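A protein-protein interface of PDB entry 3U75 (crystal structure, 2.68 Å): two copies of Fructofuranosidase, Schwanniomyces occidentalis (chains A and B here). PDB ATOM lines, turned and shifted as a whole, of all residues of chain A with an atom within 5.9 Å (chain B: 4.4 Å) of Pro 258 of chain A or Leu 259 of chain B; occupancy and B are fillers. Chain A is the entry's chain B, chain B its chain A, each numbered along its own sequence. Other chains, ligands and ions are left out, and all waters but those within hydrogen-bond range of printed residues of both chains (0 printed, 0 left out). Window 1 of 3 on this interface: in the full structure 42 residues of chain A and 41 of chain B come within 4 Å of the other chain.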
ATOM      1  N   TYR A 224      24.272 -22.355 -20.226  1.00  0.00           N
ATOM      2  CA  TYR A 224      25.359 -21.555 -19.678  1.00  0.00           C
ATOM      3  C   TYR A 224      26.688 -22.008 -20.273  1.00  0.00           C
ATOM      4  O   TYR A 224      27.020 -23.192 -20.212  1.00  0.00           O
ATOM      5  CB  TYR A 224      25.377 -21.695 -18.157  1.00  0.00           C
ATOM      6  CG  TYR A 224      25.843 -20.458 -17.422  1.00  0.00           C
ATOM      7  CD1 TYR A 224      25.112 -19.263 -17.484  1.00  0.00           C
ATOM      8  CD2 TYR A 224      27.001 -20.473 -16.651  1.00  0.00           C
ATOM      9  CE1 TYR A 224      25.537 -18.118 -16.813  1.00  0.00           C
ATOM     10  CE2 TYR A 224      27.429 -19.323 -15.972  1.00  0.00           C
ATOM     11  CZ  TYR A 224      26.691 -18.162 -16.061  1.00  0.00           C
ATOM     12  OH  TYR A 224      27.100 -17.028 -15.412  1.00  0.00           O
ATOM     13  N   ILE A 253      30.234 -28.049 -17.028  1.00  0.00           N
ATOM     14  CA  ILE A 253      31.036 -26.885 -17.348  1.00  0.00           C
ATOM     15  C   ILE A 253      31.969 -26.535 -16.220  1.00  0.00           C
ATOM     16  O   ILE A 253      31.549 -26.434 -15.067  1.00  0.00           O
ATOM     17  CB  ILE A 253      30.193 -25.665 -17.827  1.00  0.00           C
ATOM     18  CG1 ILE A 253      29.204 -25.214 -16.770  1.00  0.00           C
ATOM     19  CG2 ILE A 253      29.426 -26.004 -19.156  1.00  0.00           C
ATOM     20  CD1 ILE A 253      28.662 -23.836 -17.028  1.00  0.00           C
ATOM     21  N   GLY A 256      33.974 -21.370 -14.372  1.00  0.00           N
ATOM     22  CA  GLY A 256      32.941 -20.375 -14.651  1.00  0.00           C
ATOM     23  C   GLY A 256      31.493 -20.787 -14.389  1.00  0.00           C
ATOM     24  O   GLY A 256      30.563 -20.177 -14.951  1.00  0.00           O
ATOM     25  N   SER A 257      31.289 -21.817 -13.556  1.00  0.00           N
ATOM     26  CA  SER A 257      29.955 -22.095 -12.994  1.00  0.00           C
ATOM     27  C   SER A 257      29.447 -20.820 -12.357  1.00  0.00           C
ATOM     28  O   SER A 257      30.216 -20.144 -11.701  1.00  0.00           O
ATOM     29  CB  SER A 257      30.003 -23.146 -11.893  1.00  0.00           C
ATOM     30  OG  SER A 257      28.755 -23.227 -11.240  1.00  0.00           O
ATOM     31  N   PRO A 258      28.142 -20.515 -12.520  1.00  0.00           N
ATOM     32  CA  PRO A 258      27.699 -19.259 -11.987  1.00  0.00           C
ATOM     33  C   PRO A 258      27.841 -19.319 -10.471  1.00  0.00           C
ATOM     34  O   PRO A 258      27.929 -18.291  -9.826  1.00  0.00           O
ATOM     35  CB  PRO A 258      26.228 -19.203 -12.417  1.00  0.00           C
ATOM     36  CG  PRO A 258      25.802 -20.615 -12.449  1.00  0.00           C
ATOM     37  CD  PRO A 258      27.004 -21.385 -12.902  1.00  0.00           C
ATOM     38  N   LEU A 259      27.891 -20.529  -9.923  1.00  0.00           N
ATOM     39  CA  LEU A 259      28.100 -20.724  -8.484  1.00  0.00           C
ATOM     40  C   LEU A 259      29.568 -20.730  -8.102  1.00  0.00           C
ATOM     41  O   LEU A 259      29.888 -20.801  -6.932  1.00  0.00           O
ATOM     42  CB  LEU A 259      27.461 -22.040  -8.017  1.00  0.00           C
ATOM     43  CG  LEU A 259      26.016 -22.131  -7.530  1.00  0.00           C
ATOM     44  CD1 LEU A 259      25.004 -21.656  -8.583  1.00  0.00           C
ATOM     45  CD2 LEU A 259      25.737 -23.567  -7.200  1.00  0.00           C
ATOM     46  N   GLY A 260      30.444 -20.669  -9.096  1.00  0.00           N
ATOM     47  CA  GLY A 260      31.865 -20.722  -8.895  1.00  0.00           C
ATOM     48  C   GLY A 260      32.305 -22.114  -9.218  1.00  0.00           C
ATOM     49  O   GLY A 260      31.640 -23.065  -8.850  1.00  0.00           O
ATOM     50  N   GLY A 261      33.426 -22.227  -9.923  1.00  0.00           N
ATOM     51  CA  GLY A 261      34.000 -23.503 -10.305  1.00  0.00           C
ATOM     52  C   GLY A 261      33.197 -24.270 -11.344  1.00  0.00           C
ATOM     53  O   GLY A 261      32.952 -23.765 -12.436  1.00  0.00           O
ATOM     54  N   ILE A 263      30.038 -27.313 -12.553  1.00  0.00           N
ATOM     55  CA  ILE A 263      28.626 -27.641 -12.412  1.00  0.00           C
ATOM     56  C   ILE A 263      28.084 -28.465 -13.571  1.00  0.00           C
ATOM     57  O   ILE A 263      28.736 -28.594 -14.620  1.00  0.00           O
ATOM     58  CB  ILE A 263      27.792 -26.352 -12.222  1.00  0.00           C
ATOM     59  CG1 ILE A 263      26.365 -26.656 -11.732  1.00  0.00           C
ATOM     60  CG2 ILE A 263      27.812 -25.508 -13.476  1.00  0.00           C
ATOM     61  CD1 ILE A 263      25.772 -25.566 -10.893  1.00  0.00           C
ATOM     62  N   PHE A 285      19.988 -26.494 -14.140  1.00  0.00           N
ATOM     63  CA  PHE A 285      21.111 -27.206 -13.559  1.00  0.00           C
ATOM     64  C   PHE A 285      20.683 -28.508 -12.884  1.00  0.00           C
ATOM     65  O   PHE A 285      19.673 -28.557 -12.179  1.00  0.00           O
ATOM     66  CB  PHE A 285      21.828 -26.322 -12.527  1.00  0.00           C
ATOM     67  CG  PHE A 285      22.568 -25.137 -13.107  1.00  0.00           C
ATOM     68  CD1 PHE A 285      22.276 -23.847 -12.678  1.00  0.00           C
ATOM     69  CD2 PHE A 285      23.585 -25.313 -14.047  1.00  0.00           C
ATOM     70  CE1 PHE A 285      22.967 -22.745 -13.196  1.00  0.00           C
ATOM     71  CE2 PHE A 285      24.288 -24.191 -14.587  1.00  0.00           C
ATOM     72  CZ  PHE A 285      23.976 -22.924 -14.153  1.00  0.00           C
ATOM     73  N   SER B 257      17.055 -17.139  -8.165  1.00  0.00           N
ATOM     74  CA  SER B 257      18.314 -16.890  -8.809  1.00  0.00           C
ATOM     75  C   SER B 257      19.208 -18.060  -8.466  1.00  0.00           C
ATOM     76  O   SER B 257      19.181 -18.541  -7.326  1.00  0.00           O
ATOM     77  CB  SER B 257      18.963 -15.629  -8.284  1.00  0.00           C
ATOM     78  OG  SER B 257      20.293 -15.573  -8.752  1.00  0.00           O
ATOM     79  N   PRO B 258      20.043 -18.497  -9.431  1.00  0.00           N
ATOM     80  CA  PRO B 258      20.855 -19.671  -9.117  1.00  0.00           C
ATOM     81  C   PRO B 258      21.778 -19.383  -7.924  1.00  0.00           C
ATOM     82  O   PRO B 258      22.221 -20.333  -7.261  1.00  0.00           O
ATOM     83  CB  PRO B 258      21.654 -19.871 -10.389  1.00  0.00           C
ATOM     84  CG  PRO B 258      21.819 -18.507 -10.934  1.00  0.00           C
ATOM     85  CD  PRO B 258      20.563 -17.772 -10.611  1.00  0.00           C
ATOM     86  N   LEU B 259      22.032 -18.083  -7.677  1.00  0.00           N
ATOM     87  CA  LEU B 259      22.865 -17.604  -6.582  1.00  0.00           C
ATOM     88  C   LEU B 259      22.052 -17.417  -5.328  1.00  0.00           C
ATOM     89  O   LEU B 259      22.611 -17.104  -4.284  1.00  0.00           O
ATOM     90  CB  LEU B 259      23.530 -16.280  -6.907  1.00  0.00           C
ATOM     91  CG  LEU B 259      24.915 -16.237  -7.521  1.00  0.00           C
ATOM     92  CD1 LEU B 259      24.862 -16.885  -8.904  1.00  0.00           C
ATOM     93  CD2 LEU B 259      25.392 -14.793  -7.598  1.00  0.00           C
ATOM     94  N   GLY B 260      20.735 -17.618  -5.447  1.00  0.00           N
ATOM     95  CA  GLY B 260      19.785 -17.374  -4.364  1.00  0.00           C
ATOM     96  C   GLY B 260      19.123 -16.028  -4.531  1.00  0.00           C
ATOM     97  O   GLY B 260      19.784 -15.051  -4.835  1.00  0.00           O
ATOM     98  N   PHE B 285      24.589 -13.412 -17.169  1.00  0.00           N
ATOM     99  CA  PHE B 285      24.059 -12.575 -16.103  1.00  0.00           C
ATOM    100  C   PHE B 285      24.721 -11.197 -16.177  1.00  0.00           C
ATOM    101  O   PHE B 285      25.883 -11.081 -16.577  1.00  0.00           O
ATOM    102  CB  PHE B 285      24.309 -13.217 -14.732  1.00  0.00           C
ATOM    103  CG  PHE B 285      23.444 -14.420 -14.436  1.00  0.00           C
ATOM    104  CD1 PHE B 285      24.026 -15.658 -14.142  1.00  0.00           C
ATOM    105  CD2 PHE B 285      22.045 -14.321 -14.423  1.00  0.00           C
ATOM    106  CE1 PHE B 285      23.227 -16.793 -13.846  1.00  0.00           C
ATOM    107  CE2 PHE B 285      21.230 -15.463 -14.131  1.00  0.00           C
ATOM    108  CZ  PHE B 285      21.826 -16.694 -13.842  1.00  0.00           C
ATOM    109  N   ILE B 288      27.145 -10.714 -11.435  1.00  0.00           N
ATOM    110  CA  ILE B 288      27.229 -11.944 -10.650  1.00  0.00           C
ATOM    111  C   ILE B 288      27.450 -11.724  -9.170  1.00  0.00           C
ATOM    112  O   ILE B 288      27.827 -12.643  -8.436  1.00  0.00           O
ATOM    113  CB  ILE B 288      28.309 -12.902 -11.153  1.00  0.00           C
ATOM    114  CG1 ILE B 288      29.626 -12.188 -11.421  1.00  0.00           C
ATOM    115  CG2 ILE B 288      27.820 -13.635 -12.377  1.00  0.00           C
ATOM    116  CD1 ILE B 288      30.762 -13.164 -11.644  1.00  0.00           C
ATOM    117  N   GLY B 289      27.194 -10.502  -8.735  1.00  0.00           N
ATOM    118  CA  GLY B 289      27.146 -10.201  -7.317  1.00  0.00           C
ATOM    119  C   GLY B 289      25.774 -10.560  -6.821  1.00  0.00           C
ATOM    120  O   GLY B 289      24.921 -10.982  -7.595  1.00  0.00           O
ATOM    121  N   LYS B 290      25.550 -10.338  -5.540  1.00  0.00           N
ATOM    122  CA  LYS B 290      24.350 -10.813  -4.871  1.00  0.00           C
ATOM    123  C   LYS B 290      23.240  -9.731  -4.841  1.00  0.00           C
ATOM    124  O   LYS B 290      22.068 -10.050  -4.672  1.00  0.00           O
ATOM    125  CB  LYS B 290      24.755 -11.306  -3.454  1.00  0.00           C
ATOM    126  CG  LYS B 290      23.749 -12.118  -2.671  1.00  0.00           C
ATOM    127  CD  LYS B 290      23.712 -13.621  -2.967  1.00  0.00           C
ATOM    128  CE  LYS B 290      22.790 -14.260  -1.896  1.00  0.00           C
ATOM    129  NZ  LYS B 290      21.981 -15.448  -2.277  1.00  0.00           N
ATOM    130  N   THR B 456      24.865 -14.704   1.530  1.00  0.00           N
ATOM    131  CA  THR B 456      26.083 -15.348   1.063  1.00  0.00           C
ATOM    132  C   THR B 456      27.324 -14.486   1.339  1.00  0.00           C
ATOM    133  O   THR B 456      27.336 -13.290   1.090  1.00  0.00           O
ATOM    134  CB  THR B 456      25.968 -15.576  -0.444  1.00  0.00           C
ATOM    135  OG1 THR B 456      24.646 -16.036  -0.731  1.00  0.00           O
ATOM    136  CG2 THR B 456      27.013 -16.587  -0.968  1.00  0.00           C
ATOM    137  N   LEU B 459      31.900 -15.118  -2.839  1.00  0.00           N
ATOM    138  CA  LEU B 459      31.517 -15.208  -4.260  1.00  0.00           C
ATOM    139  C   LEU B 459      32.768 -14.959  -5.075  1.00  0.00           C
ATOM    140  O   LEU B 459      33.655 -14.229  -4.655  1.00  0.00           O
ATOM    141  CB  LEU B 459      30.476 -14.148  -4.637  1.00  0.00           C
ATOM    142  CG  LEU B 459      29.131 -14.079  -3.904  1.00  0.00           C
ATOM    143  CD1 LEU B 459      28.670 -12.651  -3.775  1.00  0.00           C
ATOM    144  CD2 LEU B 459      28.071 -14.954  -4.583  1.00  0.00           C
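Among the printed residues, pairs that only touch across the chains: Leu 259 of chain A with Pro 258 of chain B (3.4 Å), Pro 258 of chain A with Leu 259 of chain B (3.5 Å) and Tyr 224 of chain A with Phe 285 of chain B (3.6 Å).
The side-chain hydroxyl (OG) of Ser 257 of chain B lies close to the backbone NH (N) of Leu 259 of chain B, at 3.2 Å.
The backbone carbonyl oxygen (O) of Leu 259 of chain B sits at hydrogen-bond distance from the side-chain amino group (NZ) of Lys 290 of chain B (2.7 Å).
The side-chain hydroxyl (OG) of Ser 257 of chain A lies close to the backbone NH (N) of Leu 259 of chain A, 3.1 Å away.
Of the printed residues of chain B, Tyr 224 of chain A touches Phe 285 (3.6 Å).
Printed residues of chain B within 4 Å of Leu 259 of chain A: Pro 258 (3.4 Å).
Phe 285 of chain A touches none of the printed residues of chain B.
Of the printed residues of chain A, Pro 258 of chain B touches Leu 259.
Leu 259 of chain B touches one residue of chain A.
Of the printed residues of chain A, Phe 285 of chain B touches Tyr 224.
Thr 456 of chain B touches none of the printed residues of chain A.
The nearest residue of chain A that does not touch Leu 259 of chain B is Leu 259 of chain A (4.7 Å).
The nearest printed residue of chain B that does not touch Tyr 224 of chain A is Ile 288 of chain B (4.6 Å).
Pro 258 of chain A touches Leu 259 of chain B, and with the chains exchanged Leu 259 of chain A touches Pro 258 of chain B.
Of the 3 pairs that touch across the chains among the printed residues, 2 have their exchanged pair printed and touching as well.
Of the 10 printed residues of chain A, 3 touch a printed residue of chain B.
Along chain A the printed residues that touch a printed residue of chain B span positions 224 to 259.
Printed residues of chain B that touch a printed residue of chain A: Pro 258, Leu 259 and Phe 285.
Hydrophobic or aromatic side chains of chain B that line the printed part of chain A: Leu 259 and Phe 285.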
